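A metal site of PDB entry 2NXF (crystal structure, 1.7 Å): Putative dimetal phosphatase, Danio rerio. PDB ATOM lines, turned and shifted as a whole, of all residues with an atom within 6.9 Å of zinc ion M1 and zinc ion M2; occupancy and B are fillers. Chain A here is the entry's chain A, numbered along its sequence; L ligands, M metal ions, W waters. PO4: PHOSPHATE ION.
A ring nitrogen (NE2) of His 97 lies within hydrogen-bond range of the side-chain amide nitrogen of Gln 15 (3.3 Å).
The side-chain carboxylate (OD1) of Asp 63 sits at hydrogen-bond distance from the side-chain amide nitrogen (NE2) of Gln 15, 3.0 Å away.
The backbone NH (N) of His 265 is in hydrogen-bond range of the side-chain carboxylate (OD2) of Asp 13 (2.9 Å).
The backbone carbonyl oxygen of Gly 59 sits at hydrogen-bond distance from the backbone NH of Asp 13 (3.1 Å).
The side-chain amide oxygen (OD1) of Asn 96 sits close to the side-chain hydroxyl (OH) of Tyr 150, 3.4 Å away.
The side-chain hydroxyl (OH) of Tyr 100 sits at hydrogen-bond distance from the side-chain amide nitrogen (ND2) of Asn 96.
The backbone carbonyl oxygen (O) of His 228 lies within hydrogen-bond range of the backbone NH (N) of Gly 264 (3.0 Å).
NE2 of His 265 sits at hydrogen-bond distance from OD1 of Asn 198, at 2.7 Å.
Of the 24 residues printed, 4 come within 4 Å of zinc ion M1.
Zinc ion M2 is bound by OD1 of Asn 96 (2.1 Å), water W1 (2.1 Å), OD2 of Asp 60 (2.2 Å), NE2 of His 228 (2.2 Å), ND1 of His 265 (2.2 Å) and O4 of the ligand (2.5 Å).
Zinc ion M1 is bound by the side-chain amide oxygen (OE1) of Gln 15 (2.0 Å), the side-chain carboxylate (OD1) of Asp 13 (2.1 Å), water W1 (2.2 Å), an oxygen (O3) of the ligand (2.2 Å), the side-chain carboxylate (OD2) of Asp 60 (2.2 Å) and a ring nitrogen (NE2) of His 267 (2.2 Å).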
ATOM      1  N   ALA A  12     -14.291  26.806  -6.560  1.00  0.00           N
ATOM      2  CA  ALA A  12     -13.325  25.719  -6.317  1.00  0.00           C
ATOM      3  C   ALA A  12     -13.601  24.520  -7.204  1.00  0.00           C
ATOM      4  O   ALA A  12     -14.760  24.190  -7.469  1.00  0.00           O
ATOM      5  CB  ALA A  12     -13.393  25.280  -4.855  1.00  0.00           C
ATOM      6  N   ASP A  13     -12.517  23.883  -7.650  1.00  0.00           N
ATOM      7  CA  ASP A  13     -12.573  22.497  -8.182  1.00  0.00           C
ATOM      8  C   ASP A  13     -13.514  22.398  -9.383  1.00  0.00           C
ATOM      9  O   ASP A  13     -14.403  21.533  -9.434  1.00  0.00           O
ATOM     10  CB  ASP A  13     -12.944  21.479  -7.083  1.00  0.00           C
ATOM     11  CG  ASP A  13     -11.850  21.381  -6.004  1.00  0.00           C
ATOM     12  OD1 ASP A  13     -11.007  20.502  -6.115  1.00  0.00           O
ATOM     13  OD2 ASP A  13     -11.801  22.232  -5.105  1.00  0.00           O
ATOM     14  N   VAL A  14     -13.317  23.306 -10.350  1.00  0.00           N
ATOM     15  CA  VAL A  14     -14.054  23.249 -11.631  1.00  0.00           C
ATOM     16  C   VAL A  14     -13.775  21.878 -12.293  1.00  0.00           C
ATOM     17  O   VAL A  14     -14.694  21.152 -12.670  1.00  0.00           O
ATOM     18  CB  VAL A  14     -13.656  24.426 -12.550  1.00  0.00           C
ATOM     19  CG1 VAL A  14     -14.343  24.298 -13.928  1.00  0.00           C
ATOM     20  CG2 VAL A  14     -14.015  25.782 -11.905  1.00  0.00           C
ATOM     21  N   GLN A  15     -12.493  21.531 -12.405  1.00  0.00           N
ATOM     22  CA  GLN A  15     -12.063  20.214 -12.882  1.00  0.00           C
ATOM     23  C   GLN A  15     -12.666  19.846 -14.233  1.00  0.00           C
ATOM     24  O   GLN A  15     -13.095  18.709 -14.455  1.00  0.00           O
ATOM     25  CB  GLN A  15     -12.306  19.102 -11.828  1.00  0.00           C
ATOM     26  CG  GLN A  15     -11.021  18.809 -11.084  1.00  0.00           C
ATOM     27  CD  GLN A  15     -11.196  18.040  -9.803  1.00  0.00           C
ATOM     28  OE1 GLN A  15     -11.289  18.631  -8.720  1.00  0.00           O
ATOM     29  NE2 GLN A  15     -11.247  16.721  -9.911  1.00  0.00           N
ATOM     30  N   ARG A  31     -19.117  12.942 -11.060  1.00  0.00           N
ATOM     31  CA  ARG A  31     -18.276  14.042 -11.546  1.00  0.00           C
ATOM     32  C   ARG A  31     -18.754  14.533 -12.924  1.00  0.00           C
ATOM     33  O   ARG A  31     -18.788  13.771 -13.885  1.00  0.00           O
ATOM     34  CB  ARG A  31     -16.794  13.649 -11.525  1.00  0.00           C
ATOM     35  CG  ARG A  31     -16.313  13.649 -10.085  1.00  0.00           C
ATOM     36  CD  ARG A  31     -14.861  13.404  -9.875  1.00  0.00           C
ATOM     37  NE  ARG A  31     -14.606  13.371  -8.429  1.00  0.00           N
ATOM     38  CZ  ARG A  31     -13.402  13.469  -7.869  1.00  0.00           C
ATOM     39  NH1 ARG A  31     -12.308  13.630  -8.624  1.00  0.00           N
ATOM     40  NH2 ARG A  31     -13.301  13.410  -6.546  1.00  0.00           N
ATOM     41  N   LEU A  58      -9.807  28.243  -6.420  1.00  0.00           N
ATOM     42  CA  LEU A  58      -9.085  27.490  -5.408  1.00  0.00           C
ATOM     43  C   LEU A  58      -8.375  26.226  -5.936  1.00  0.00           C
ATOM     44  O   LEU A  58      -7.882  25.416  -5.145  1.00  0.00           O
ATOM     45  CB  LEU A  58     -10.046  27.132  -4.261  1.00  0.00           C
ATOM     46  CG  LEU A  58     -10.262  28.195  -3.149  1.00  0.00           C
ATOM     47  CD1 LEU A  58      -8.945  28.437  -2.382  1.00  0.00           C
ATOM     48  CD2 LEU A  58     -10.757  29.474  -3.716  1.00  0.00           C
ATOM     49  N   GLY A  59      -8.283  26.080  -7.269  1.00  0.00           N
ATOM     50  CA  GLY A  59      -7.446  25.016  -7.841  1.00  0.00           C
ATOM     51  C   GLY A  59      -8.284  23.874  -8.384  1.00  0.00           C
ATOM     52  O   GLY A  59      -9.514  23.868  -8.266  1.00  0.00           O
ATOM     53  N   ASP A  60      -7.571  22.871  -8.919  1.00  0.00           N
ATOM     54  CA  ASP A  60      -8.180  21.791  -9.683  1.00  0.00           C
ATOM     55  C   ASP A  60      -9.087  22.374 -10.747  1.00  0.00           C
ATOM     56  O   ASP A  60     -10.233  21.934 -10.892  1.00  0.00           O
ATOM     57  CB  ASP A  60      -8.980  20.850  -8.778  1.00  0.00           C
ATOM     58  CG  ASP A  60      -8.105  19.948  -7.914  1.00  0.00           C
ATOM     59  OD1 ASP A  60      -6.861  20.015  -8.001  1.00  0.00           O
ATOM     60  OD2 ASP A  60      -8.654  19.214  -7.094  1.00  0.00           O
ATOM     61  N   ASP A  63      -9.330  18.767 -14.966  1.00  0.00           N
ATOM     62  CA  ASP A  63      -9.127  17.442 -14.365  1.00  0.00           C
ATOM     63  C   ASP A  63      -7.850  16.778 -14.868  1.00  0.00           C
ATOM     64  O   ASP A  63      -7.458  16.983 -16.024  1.00  0.00           O
ATOM     65  CB  ASP A  63     -10.316  16.530 -14.658  1.00  0.00           C
ATOM     66  CG  ASP A  63     -10.373  15.336 -13.735  1.00  0.00           C
ATOM     67  OD1 ASP A  63     -10.836  15.506 -12.586  1.00  0.00           O
ATOM     68  OD2 ASP A  63      -9.930  14.262 -14.136  1.00  0.00           O
ATOM     69  N   GLY A  95      -3.695  23.262  -7.326  1.00  0.00           N
ATOM     70  CA  GLY A  95      -4.055  22.030  -6.605  1.00  0.00           C
ATOM     71  C   GLY A  95      -3.513  20.773  -7.258  1.00  0.00           C
ATOM     72  O   GLY A  95      -2.736  20.814  -8.237  1.00  0.00           O
ATOM     73  N   ASN A  96      -3.896  19.622  -6.715  1.00  0.00           N
ATOM     74  CA  ASN A  96      -3.365  18.349  -7.229  1.00  0.00           C
ATOM     75  C   ASN A  96      -3.582  18.129  -8.722  1.00  0.00           C
ATOM     76  O   ASN A  96      -2.679  17.649  -9.400  1.00  0.00           O
ATOM     77  CB  ASN A  96      -3.756  17.109  -6.397  1.00  0.00           C
ATOM     78  CG  ASN A  96      -5.251  17.007  -6.142  1.00  0.00           C
ATOM     79  OD1 ASN A  96      -5.899  17.972  -5.752  1.00  0.00           O
ATOM     80  ND2 ASN A  96      -5.800  15.808  -6.370  1.00  0.00           N
ATOM     81  N   HIS A  97      -4.743  18.518  -9.255  1.00  0.00           N
ATOM     82  CA  HIS A  97      -5.016  18.297 -10.681  1.00  0.00           C
ATOM     83  C   HIS A  97      -4.182  19.164 -11.604  1.00  0.00           C
ATOM     84  O   HIS A  97      -3.866  18.765 -12.733  1.00  0.00           O
ATOM     85  CB  HIS A  97      -6.515  18.364 -10.960  1.00  0.00           C
ATOM     86  CG  HIS A  97      -7.239  17.152 -10.475  1.00  0.00           C
ATOM     87  ND1 HIS A  97      -7.567  16.106 -11.311  1.00  0.00           N
ATOM     88  CD2 HIS A  97      -7.609  16.768  -9.233  1.00  0.00           C
ATOM     89  CE1 HIS A  97      -8.148  15.149 -10.615  1.00  0.00           C
ATOM     90  NE2 HIS A  97      -8.181  15.521  -9.351  1.00  0.00           N
ATOM     91  N   TYR A 100      -1.096  17.071 -11.878  1.00  0.00           N
ATOM     92  CA  TYR A 100      -1.314  15.886 -12.710  1.00  0.00           C
ATOM     93  C   TYR A 100      -1.146  16.255 -14.181  1.00  0.00           C
ATOM     94  O   TYR A 100      -0.646  15.456 -14.962  1.00  0.00           O
ATOM     95  CB  TYR A 100      -2.721  15.300 -12.530  1.00  0.00           C
ATOM     96  CG  TYR A 100      -3.051  14.812 -11.126  1.00  0.00           C
ATOM     97  CD1 TYR A 100      -2.054  14.345 -10.261  1.00  0.00           C
ATOM     98  CD2 TYR A 100      -4.377  14.779 -10.692  1.00  0.00           C
ATOM     99  CE1 TYR A 100      -2.367  13.899  -8.971  1.00  0.00           C
ATOM    100  CE2 TYR A 100      -4.714  14.332  -9.411  1.00  0.00           C
ATOM    101  CZ  TYR A 100      -3.704  13.905  -8.553  1.00  0.00           C
ATOM    102  OH  TYR A 100      -4.044  13.501  -7.283  1.00  0.00           O
ATOM    103  N   TYR A 150       1.240  22.070  -2.203  1.00  0.00           N
ATOM    104  CA  TYR A 150       2.046  20.968  -2.790  1.00  0.00           C
ATOM    105  C   TYR A 150       3.541  21.294  -2.846  1.00  0.00           C
ATOM    106  O   TYR A 150       4.300  20.663  -3.572  1.00  0.00           O
ATOM    107  CB  TYR A 150       1.488  20.537  -4.167  1.00  0.00           C
ATOM    108  CG  TYR A 150       0.116  19.962  -3.988  1.00  0.00           C
ATOM    109  CD1 TYR A 150      -0.071  18.583  -3.786  1.00  0.00           C
ATOM    110  CD2 TYR A 150      -1.009  20.805  -3.899  1.00  0.00           C
ATOM    111  CE1 TYR A 150      -1.337  18.058  -3.563  1.00  0.00           C
ATOM    112  CE2 TYR A 150      -2.278  20.287  -3.683  1.00  0.00           C
ATOM    113  CZ  TYR A 150      -2.440  18.921  -3.493  1.00  0.00           C
ATOM    114  OH  TYR A 150      -3.678  18.364  -3.269  1.00  0.00           O
ATOM    115  N   PHE A 197      -2.270  12.310  -3.125  1.00  0.00           N
ATOM    116  CA  PHE A 197      -3.011  13.453  -3.670  1.00  0.00           C
ATOM    117  C   PHE A 197      -3.055  14.678  -2.738  1.00  0.00           C
ATOM    118  O   PHE A 197      -3.668  15.683  -3.069  1.00  0.00           O
ATOM    119  CB  PHE A 197      -4.402  13.042  -4.163  1.00  0.00           C
ATOM    120  CG  PHE A 197      -5.308  12.446  -3.114  1.00  0.00           C
ATOM    121  CD1 PHE A 197      -6.050  13.276  -2.252  1.00  0.00           C
ATOM    122  CD2 PHE A 197      -5.509  11.062  -3.051  1.00  0.00           C
ATOM    123  CE1 PHE A 197      -6.958  12.743  -1.318  1.00  0.00           C
ATOM    124  CE2 PHE A 197      -6.425  10.502  -2.112  1.00  0.00           C
ATOM    125  CZ  PHE A 197      -7.140  11.337  -1.255  1.00  0.00           C
ATOM    126  N   ASN A 198      -2.399  14.565  -1.581  1.00  0.00           N
ATOM    127  CA  ASN A 198      -2.195  15.690  -0.687  1.00  0.00           C
ATOM    128  C   ASN A 198      -0.731  16.150  -0.674  1.00  0.00           C
ATOM    129  O   ASN A 198       0.109  15.641  -1.422  1.00  0.00           O
ATOM    130  CB  ASN A 198      -2.684  15.383   0.731  1.00  0.00           C
ATOM    131  CG  ASN A 198      -4.174  15.177   0.794  1.00  0.00           C
ATOM    132  OD1 ASN A 198      -4.922  15.689  -0.058  1.00  0.00           O
ATOM    133  ND2 ASN A 198      -4.629  14.465   1.816  1.00  0.00           N
ATOM    134  N   HIS A 228      -5.111  25.243  -1.700  1.00  0.00           N
ATOM    135  CA  HIS A 228      -5.987  24.219  -2.284  1.00  0.00           C
ATOM    136  C   HIS A 228      -6.494  23.318  -1.141  1.00  0.00           C
ATOM    137  O   HIS A 228      -7.668  22.921  -1.136  1.00  0.00           O
ATOM    138  CB  HIS A 228      -5.270  23.345  -3.307  1.00  0.00           C
ATOM    139  CG  HIS A 228      -6.181  22.384  -3.977  1.00  0.00           C
ATOM    140  ND1 HIS A 228      -7.277  22.792  -4.715  1.00  0.00           N
ATOM    141  CD2 HIS A 228      -6.194  21.025  -3.990  1.00  0.00           C
ATOM    142  CE1 HIS A 228      -7.904  21.719  -5.173  1.00  0.00           C
ATOM    143  NE2 HIS A 228      -7.268  20.641  -4.746  1.00  0.00           N
ATOM    144  N   LEU A 229      -5.607  23.020  -0.202  1.00  0.00           N
ATOM    145  CA  LEU A 229      -5.911  22.083   0.883  1.00  0.00           C
ATOM    146  C   LEU A 229      -6.364  22.770   2.166  1.00  0.00           C
ATOM    147  O   LEU A 229      -5.748  23.746   2.615  1.00  0.00           O
ATOM    148  CB  LEU A 229      -4.676  21.232   1.234  1.00  0.00           C
ATOM    149  CG  LEU A 229      -4.141  20.315   0.112  1.00  0.00           C
ATOM    150  CD1 LEU A 229      -2.893  19.546   0.609  1.00  0.00           C
ATOM    151  CD2 LEU A 229      -5.204  19.381  -0.377  1.00  0.00           C
ATOM    152  N   GLY A 264     -10.201  24.547  -1.114  1.00  0.00           N
ATOM    153  CA  GLY A 264     -11.073  23.696  -1.939  1.00  0.00           C
ATOM    154  C   GLY A 264     -10.752  22.264  -1.564  1.00  0.00           C
ATOM    155  O   GLY A 264     -10.628  21.927  -0.370  1.00  0.00           O
ATOM    156  N   HIS A 265     -10.603  21.419  -2.579  1.00  0.00           N
ATOM    157  CA  HIS A 265     -10.132  20.015  -2.462  1.00  0.00           C
ATOM    158  C   HIS A 265     -11.187  19.056  -1.938  1.00  0.00           C
ATOM    159  O   HIS A 265     -11.432  18.022  -2.563  1.00  0.00           O
ATOM    160  CB  HIS A 265      -8.812  19.908  -1.666  1.00  0.00           C
ATOM    161  CG  HIS A 265      -8.106  18.589  -1.792  1.00  0.00           C
ATOM    162  ND1 HIS A 265      -7.625  18.090  -2.987  1.00  0.00           N
ATOM    163  CD2 HIS A 265      -7.697  17.713  -0.839  1.00  0.00           C
ATOM    164  CE1 HIS A 265      -6.984  16.956  -2.777  1.00  0.00           C
ATOM    165  NE2 HIS A 265      -7.011  16.693  -1.474  1.00  0.00           N
ATOM    166  N   ASP A 266     -11.778  19.358  -0.777  1.00  0.00           N
ATOM    167  CA  ASP A 266     -12.866  18.503  -0.280  1.00  0.00           C
ATOM    168  C   ASP A 266     -14.143  18.986  -0.958  1.00  0.00           C
ATOM    169  O   ASP A 266     -14.719  20.006  -0.550  1.00  0.00           O
ATOM    170  CB  ASP A 266     -12.978  18.616   1.253  1.00  0.00           C
ATOM    171  CG  ASP A 266     -14.072  17.756   1.840  1.00  0.00           C
ATOM    172  OD1 ASP A 266     -14.868  17.155   1.076  1.00  0.00           O
ATOM    173  OD2 ASP A 266     -14.127  17.648   3.079  1.00  0.00           O
ATOM    174  N   HIS A 267     -14.582  18.256  -1.987  1.00  0.00           N
ATOM    175  CA  HIS A 267     -15.701  18.727  -2.830  1.00  0.00           C
ATOM    176  C   HIS A 267     -17.017  18.824  -2.074  1.00  0.00           C
ATOM    177  O   HIS A 267     -17.936  19.482  -2.529  1.00  0.00           O
ATOM    178  CB  HIS A 267     -15.892  17.819  -4.045  1.00  0.00           C
ATOM    179  CG  HIS A 267     -14.672  17.709  -4.915  1.00  0.00           C
ATOM    180  ND1 HIS A 267     -14.432  16.616  -5.733  1.00  0.00           N
ATOM    181  CD2 HIS A 267     -13.639  18.568  -5.112  1.00  0.00           C
ATOM    182  CE1 HIS A 267     -13.297  16.806  -6.381  1.00  0.00           C
ATOM    183  NE2 HIS A 267     -12.788  17.980  -6.027  1.00  0.00           N
ATOM    184  N   GLY A 285     -17.274  21.748  -4.214  1.00  0.00           N
ATOM    185  CA  GLY A 285     -16.580  21.689  -5.515  1.00  0.00           C
ATOM    186  C   GLY A 285     -17.547  21.673  -6.677  1.00  0.00           C
ATOM    187  O   GLY A 285     -18.559  20.944  -6.683  1.00  0.00           O
ATOM    188  N   ILE A 287     -17.044  20.451  -9.610  1.00  0.00           N
ATOM    189  CA  ILE A 287     -17.057  19.167 -10.339  1.00  0.00           C
ATOM    190  C   ILE A 287     -18.104  18.177  -9.852  1.00  0.00           C
ATOM    191  O   ILE A 287     -18.629  17.402 -10.652  1.00  0.00           O
ATOM    192  CB  ILE A 287     -15.647  18.537 -10.382  1.00  0.00           C
ATOM    193  CG1 ILE A 287     -15.605  17.301 -11.295  1.00  0.00           C
ATOM    194  CG2 ILE A 287     -15.144  18.203  -8.964  1.00  0.00           C
ATOM    195  CD1 ILE A 287     -15.912  17.601 -12.764  1.00  0.00           C
HETATM  196  P   PO4 L   1      -9.650  15.477  -6.234  1.00  0.00           P
HETATM  197  O1  PO4 L   1     -10.477  15.040  -5.041  1.00  0.00           O
HETATM  198  O2  PO4 L   1      -9.367  14.278  -7.107  1.00  0.00           O
HETATM  199  O3  PO4 L   1     -10.425  16.431  -7.142  1.00  0.00           O
HETATM  200  O4  PO4 L   1      -8.398  16.161  -5.800  1.00  0.00           O
HETATM  201 ZN    ZN M   1     -10.761  18.566  -6.801  1.00  0.00          ZN
HETATM  202 ZN    ZN M   2      -7.871  18.559  -5.169  1.00  0.00          ZN
HETATM  203  O   HOH W   1      -9.934  18.047  -4.883  1.00  0.00           O
